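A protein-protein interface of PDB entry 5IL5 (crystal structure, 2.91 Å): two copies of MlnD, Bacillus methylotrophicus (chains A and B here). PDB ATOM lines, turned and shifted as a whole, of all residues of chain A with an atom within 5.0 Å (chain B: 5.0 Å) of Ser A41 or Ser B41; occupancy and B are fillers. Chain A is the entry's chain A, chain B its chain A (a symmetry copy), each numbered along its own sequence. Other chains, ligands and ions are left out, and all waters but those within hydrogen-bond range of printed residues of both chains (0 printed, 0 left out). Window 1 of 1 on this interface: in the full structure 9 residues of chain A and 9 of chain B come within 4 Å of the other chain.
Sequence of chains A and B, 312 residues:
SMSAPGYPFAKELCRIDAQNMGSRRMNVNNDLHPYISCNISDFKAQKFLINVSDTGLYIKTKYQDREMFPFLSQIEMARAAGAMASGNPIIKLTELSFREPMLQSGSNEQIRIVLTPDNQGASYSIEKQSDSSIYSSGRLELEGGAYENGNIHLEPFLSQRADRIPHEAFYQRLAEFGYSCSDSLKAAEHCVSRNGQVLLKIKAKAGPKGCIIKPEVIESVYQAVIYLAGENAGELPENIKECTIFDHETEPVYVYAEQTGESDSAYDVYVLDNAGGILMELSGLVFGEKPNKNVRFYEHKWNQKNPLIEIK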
ATOM      1  N   ASN A  39     -13.214 -17.705 -11.533  1.00  0.00           N
ATOM      2  CA  ASN A  39     -12.009 -16.978 -11.914  1.00  0.00           C
ATOM      3  C   ASN A  39     -11.009 -17.963 -12.511  1.00  0.00           C
ATOM      4  O   ASN A  39     -10.656 -18.957 -11.870  1.00  0.00           O
ATOM      5  CB  ASN A  39     -11.421 -16.256 -10.701  1.00  0.00           C
ATOM      6  CG  ASN A  39     -10.180 -15.460 -11.037  1.00  0.00           C
ATOM      7  OD1 ASN A  39      -9.502 -15.720 -12.033  1.00  0.00           O
ATOM      8  ND2 ASN A  39      -9.894 -14.454 -10.222  1.00  0.00           N
ATOM      9  N   ILE A  40     -10.581 -17.698 -13.747  1.00  0.00           N
ATOM     10  CA  ILE A  40      -9.637 -18.565 -14.448  1.00  0.00           C
ATOM     11  C   ILE A  40      -8.372 -17.802 -14.824  1.00  0.00           C
ATOM     12  O   ILE A  40      -7.739 -18.091 -15.844  1.00  0.00           O
ATOM     13  CB  ILE A  40     -10.298 -19.172 -15.697  1.00  0.00           C
ATOM     14  CG1 ILE A  40     -10.988 -18.074 -16.516  1.00  0.00           C
ATOM     15  CG2 ILE A  40     -11.283 -20.243 -15.274  1.00  0.00           C
ATOM     16  CD1 ILE A  40     -11.177 -18.411 -17.976  1.00  0.00           C
ATOM     17  N   SER A  41      -7.995 -16.836 -13.996  1.00  0.00           N
ATOM     18  CA  SER A  41      -6.798 -16.045 -14.245  1.00  0.00           C
ATOM     19  C   SER A  41      -5.548 -16.915 -14.202  1.00  0.00           C
ATOM     20  O   SER A  41      -5.515 -17.963 -13.553  1.00  0.00           O
ATOM     21  CB  SER A  41      -6.688 -14.931 -13.212  1.00  0.00           C
ATOM     22  OG  SER A  41      -7.871 -14.160 -13.173  1.00  0.00           O
ATOM     23  N   ASP A  42      -4.512 -16.481 -14.918  1.00  0.00           N
ATOM     24  CA  ASP A  42      -3.220 -17.154 -14.885  1.00  0.00           C
ATOM     25  C   ASP A  42      -2.121 -16.121 -15.111  1.00  0.00           C
ATOM     26  O   ASP A  42      -2.382 -14.920 -15.246  1.00  0.00           O
ATOM     27  CB  ASP A  42      -3.151 -18.283 -15.921  1.00  0.00           C
ATOM     28  CG  ASP A  42      -3.352 -17.785 -17.350  1.00  0.00           C
ATOM     29  OD1 ASP A  42      -3.018 -16.615 -17.634  1.00  0.00           O
ATOM     30  OD2 ASP A  42      -3.847 -18.567 -18.193  1.00  0.00           O
ATOM     31  N   PHE A  43      -0.879 -16.606 -15.181  1.00  0.00           N
ATOM     32  CA  PHE A  43       0.255 -15.704 -15.351  1.00  0.00           C
ATOM     33  C   PHE A  43       0.106 -14.881 -16.611  1.00  0.00           C
ATOM     34  O   PHE A  43       0.537 -13.723 -16.658  1.00  0.00           O
ATOM     35  CB  PHE A  43       1.552 -16.507 -15.425  1.00  0.00           C
ATOM     36  CG  PHE A  43       2.002 -17.065 -14.111  1.00  0.00           C
ATOM     37  CD1 PHE A  43       1.798 -16.379 -12.931  1.00  0.00           C
ATOM     38  CD2 PHE A  43       2.611 -18.306 -14.063  1.00  0.00           C
ATOM     39  CE1 PHE A  43       2.216 -16.910 -11.733  1.00  0.00           C
ATOM     40  CE2 PHE A  43       3.028 -18.839 -12.871  1.00  0.00           C
ATOM     41  CZ  PHE A  43       2.827 -18.139 -11.700  1.00  0.00           C
ATOM     42  N   ALA A  45      -2.739 -13.838 -18.193  1.00  0.00           N
ATOM     43  CA  ALA A  45      -3.705 -12.756 -18.098  1.00  0.00           C
ATOM     44  C   ALA A  45      -4.754 -13.027 -17.024  1.00  0.00           C
ATOM     45  O   ALA A  45      -5.098 -14.175 -16.731  1.00  0.00           O
ATOM     46  CB  ALA A  45      -4.373 -12.522 -19.457  1.00  0.00           C
ATOM     47  N   GLN A  46      -5.261 -11.931 -16.462  1.00  0.00           N
ATOM     48  CA  GLN A  46      -6.428 -11.957 -15.592  1.00  0.00           C
ATOM     49  C   GLN A  46      -7.686 -12.239 -16.405  1.00  0.00           C
ATOM     50  O   GLN A  46      -7.913 -11.617 -17.447  1.00  0.00           O
ATOM     51  CB  GLN A  46      -6.550 -10.610 -14.888  1.00  0.00           C
ATOM     52  CG  GLN A  46      -7.799 -10.404 -14.056  1.00  0.00           C
ATOM     53  CD  GLN A  46      -7.718 -11.020 -12.665  1.00  0.00           C
ATOM     54  OE1 GLN A  46      -6.638 -11.154 -12.093  1.00  0.00           O
ATOM     55  NE2 GLN A  46      -8.868 -11.389 -12.113  1.00  0.00           N
ATOM     56  N   LYS A  47      -8.516 -13.169 -15.937  1.00  0.00           N
ATOM     57  CA  LYS A  47      -9.686 -13.491 -16.742  1.00  0.00           C
ATOM     58  C   LYS A  47     -10.669 -14.343 -15.954  1.00  0.00           C
ATOM     59  O   LYS A  47     -10.289 -15.055 -15.020  1.00  0.00           O
ATOM     60  CB  LYS A  47      -9.256 -14.205 -18.023  1.00  0.00           C
ATOM     61  CG  LYS A  47      -8.300 -15.355 -17.775  1.00  0.00           C
ATOM     62  CD  LYS A  47      -7.709 -15.863 -19.061  1.00  0.00           C
ATOM     63  CE  LYS A  47      -6.487 -16.696 -18.777  1.00  0.00           C
ATOM     64  NZ  LYS A  47      -6.073 -17.466 -19.965  1.00  0.00           N
ATOM     65  N   ASN B  39      -9.772 -19.939  -7.298  1.00  0.00           N
ATOM     66  CA  ASN B  39      -8.805 -18.962  -7.783  1.00  0.00           C
ATOM     67  C   ASN B  39      -9.281 -17.566  -7.395  1.00  0.00           C
ATOM     68  O   ASN B  39     -10.403 -17.175  -7.729  1.00  0.00           O
ATOM     69  CB  ASN B  39      -8.637 -19.091  -9.297  1.00  0.00           C
ATOM     70  CG  ASN B  39      -7.625 -18.119  -9.860  1.00  0.00           C
ATOM     71  OD1 ASN B  39      -7.321 -17.089  -9.255  1.00  0.00           O
ATOM     72  ND2 ASN B  39      -7.065 -18.461 -11.012  1.00  0.00           N
ATOM     73  N   ILE B  40      -8.437 -16.833  -6.666  1.00  0.00           N
ATOM     74  CA  ILE B  40      -8.768 -15.485  -6.209  1.00  0.00           C
ATOM     75  C   ILE B  40      -7.764 -14.468  -6.737  1.00  0.00           C
ATOM     76  O   ILE B  40      -7.481 -13.459  -6.083  1.00  0.00           O
ATOM     77  CB  ILE B  40      -8.828 -15.443  -4.673  1.00  0.00           C
ATOM     78  CG1 ILE B  40      -7.576 -16.101  -4.077  1.00  0.00           C
ATOM     79  CG2 ILE B  40     -10.091 -16.135  -4.200  1.00  0.00           C
ATOM     80  CD1 ILE B  40      -7.242 -15.650  -2.675  1.00  0.00           C
ATOM     81  N   SER B  41      -7.233 -14.722  -7.928  1.00  0.00           N
ATOM     82  CA  SER B  41      -6.270 -13.818  -8.540  1.00  0.00           C
ATOM     83  C   SER B  41      -6.900 -12.461  -8.830  1.00  0.00           C
ATOM     84  O   SER B  41      -8.114 -12.341  -9.009  1.00  0.00           O
ATOM     85  CB  SER B  41      -5.736 -14.426  -9.830  1.00  0.00           C
ATOM     86  OG  SER B  41      -5.222 -15.723  -9.602  1.00  0.00           O
ATOM     87  N   ASP B  42      -6.062 -11.426  -8.861  1.00  0.00           N
ATOM     88  CA  ASP B  42      -6.509 -10.089  -9.231  1.00  0.00           C
ATOM     89  C   ASP B  42      -5.354  -9.354  -9.904  1.00  0.00           C
ATOM     90  O   ASP B  42      -4.264  -9.905 -10.100  1.00  0.00           O
ATOM     91  CB  ASP B  42      -7.032  -9.317  -8.014  1.00  0.00           C
ATOM     92  CG  ASP B  42      -5.976  -9.143  -6.927  1.00  0.00           C
ATOM     93  OD1 ASP B  42      -4.770  -9.107  -7.256  1.00  0.00           O
ATOM     94  OD2 ASP B  42      -6.351  -9.045  -5.736  1.00  0.00           O
ATOM     95  N   PHE B  43      -5.593  -8.083 -10.234  1.00  0.00           N
ATOM     96  CA  PHE B  43      -4.575  -7.296 -10.921  1.00  0.00           C
ATOM     97  C   PHE B  43      -3.300  -7.236 -10.110  1.00  0.00           C
ATOM     98  O   PHE B  43      -2.200  -7.193 -10.674  1.00  0.00           O
ATOM     99  CB  PHE B  43      -5.087  -5.878 -11.161  1.00  0.00           C
ATOM    100  CG  PHE B  43      -6.114  -5.771 -12.245  1.00  0.00           C
ATOM    101  CD1 PHE B  43      -6.064  -6.578 -13.363  1.00  0.00           C
ATOM    102  CD2 PHE B  43      -7.156  -4.870 -12.121  1.00  0.00           C
ATOM    103  CE1 PHE B  43      -7.019  -6.468 -14.348  1.00  0.00           C
ATOM    104  CE2 PHE B  43      -8.109  -4.759 -13.099  1.00  0.00           C
ATOM    105  CZ  PHE B  43      -8.042  -5.564 -14.216  1.00  0.00           C
ATOM    106  N   ALA B  45      -2.028  -9.514  -7.901  1.00  0.00           N
ATOM    107  CA  ALA B  45      -1.237 -10.732  -7.927  1.00  0.00           C
ATOM    108  C   ALA B  45      -2.093 -11.956  -8.242  1.00  0.00           C
ATOM    109  O   ALA B  45      -3.284 -12.011  -7.923  1.00  0.00           O
ATOM    110  CB  ALA B  45      -0.505 -10.915  -6.594  1.00  0.00           C
ATOM    111  N   GLN B  46      -1.441 -12.938  -8.861  1.00  0.00           N
ATOM    112  CA  GLN B  46      -2.003 -14.269  -9.042  1.00  0.00           C
ATOM    113  C   GLN B  46      -2.047 -15.007  -7.710  1.00  0.00           C
ATOM    114  O   GLN B  46      -1.057 -15.032  -6.972  1.00  0.00           O
ATOM    115  CB  GLN B  46      -1.144 -15.037 -10.040  1.00  0.00           C
ATOM    116  CG  GLN B  46      -1.495 -16.497 -10.234  1.00  0.00           C
ATOM    117  CD  GLN B  46      -2.654 -16.728 -11.195  1.00  0.00           C
ATOM    118  OE1 GLN B  46      -2.892 -15.934 -12.103  1.00  0.00           O
ATOM    119  NE2 GLN B  46      -3.374 -17.826 -11.001  1.00  0.00           N
ATOM    120  N   LYS B  47      -3.185 -15.622  -7.393  1.00  0.00           N
ATOM    121  CA  LYS B  47      -3.257 -16.274  -6.093  1.00  0.00           C
ATOM    122  C   LYS B  47      -4.489 -17.159  -5.998  1.00  0.00           C
ATOM    123  O   LYS B  47      -5.490 -16.935  -6.684  1.00  0.00           O
ATOM    124  CB  LYS B  47      -3.258 -15.223  -4.983  1.00  0.00           C
ATOM    125  CG  LYS B  47      -4.265 -14.113  -5.210  1.00  0.00           C
ATOM    126  CD  LYS B  47      -4.061 -12.982  -4.241  1.00  0.00           C
ATOM    127  CE  LYS B  47      -4.770 -11.746  -4.730  1.00  0.00           C
ATOM    128  NZ  LYS B  47      -4.865 -10.725  -3.670  1.00  0.00           N
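Of the 8 printed residues of chain B, 5 touch a printed residue of chain A. Among the printed residues, no Asp or Glu carboxylate lies within 4 Å of a Lys or Arg side-chain nitrogen of the other chain.
Of the printed residues of chain B, Asn A39 touches Asn B39 (3.3 Å) and Ser B41 (3.0 Å). Of the printed residues of chain B, Ser A41 touches Asn B39, Ser B41 and Gln B46. Printed residues of chain B within 4 Å of Phe A43: Gln B46 (3.7 Å). Ala A45 touches none of the printed residues of chain B. Printed residues of chain A within 4 Å of Ser B41: Asn A39 (3.0 Å), Ser A41 (3.5 Å) and Gln A46 (3.3 Å). Printed residues of chain A within 4 Å of Asp B42: Gln A46. Of the printed residues of chain A, Phe B43 touches Gln A46 (3.7 Å). Of the printed residues of chain A, Gln B46 touches Ser A41 (3.3 Å), Asp A42 (3.1 Å) and Phe A43 (3.7 Å). The nearest printed residue of chain B that does not touch Ser A41 is Asp B42 (5.4 Å). The nearest printed residue of chain A that does not touch Ser B41 is Asp A42 (5.4 Å). The nearest printed residue of chain B that does not touch Gln A46 is Ala B45 (5.4 Å).
Asn A39 touches Asn B39 (CB to O, 3.3 Å). Ser A41 touches Ser B41 (CB to CB, 3.5 Å). Phe A43 touches Gln B46 (N to OE1, 3.7 Å). N of Phe B43 touches OE1 of Gln A46, 3.7 Å away.
O of Ser B41 lies within hydrogen-bond range of ND2 of Asn A39, 3.0 Å away. The backbone carbonyl oxygen of Ser A41 sits at hydrogen-bond distance from the side-chain amide nitrogen of Asn B39 (3.0 Å). The backbone carbonyl oxygen (O) of Ser A41 sits at hydrogen-bond distance from the side-chain amide nitrogen (NE2) of Gln B46 (3.3 Å). The side-chain amide oxygen (OE1) of Gln B46 lies close to the backbone NH (N) of Asp A42, 3.3 Å away. The side-chain amide nitrogen of Gln A46 lies within hydrogen-bond range of the backbone carbonyl oxygen of Ser B41 (3.3 Å). The side-chain amide oxygen (OE1) of Gln A46 sits close to the backbone NH (N) of Asp B42, at 3.3 Å.
Asn B39 touches its own counterpart, Asn A39. Asn A39 touches Ser B41, and with the chains exchanged Ser A41 touches Asn B39. Ser B41 touches its own counterpart, Ser A41. Ser A41 touches Gln B46, and with the chains exchanged Gln A46 touches Ser B41. 8 positions are printed for both chains. Of the 10 pairs that touch across the chains among the printed residues, 10 have their exchanged pair printed and touching as well.
OD1 of Asn A39 lies close to O of Lys A47 (3.2 Å). The side-chain amide nitrogen (NE2) of Gln A46 is in hydrogen-bond range of the side-chain hydroxyl (OG) of Ser A41, 3.1 Å away. The side-chain hydroxyl (OG) of Ser A41 lies within hydrogen-bond range of the backbone NH (N) of Lys A47, at 3.0 Å. The side-chain carboxylate (OD2) of Asp A42 is in salt-bridge range of the side-chain amino group (NZ) of Lys A47, 3.1 Å away. OD1 of Asp B42 lies within hydrogen-bond range of N of Ala B45 (2.8 Å). The side-chain amino group (NZ) of Lys B47 lies within salt-bridge range of the side-chain carboxylate (OD2) of Asp B42, at 3.0 Å.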
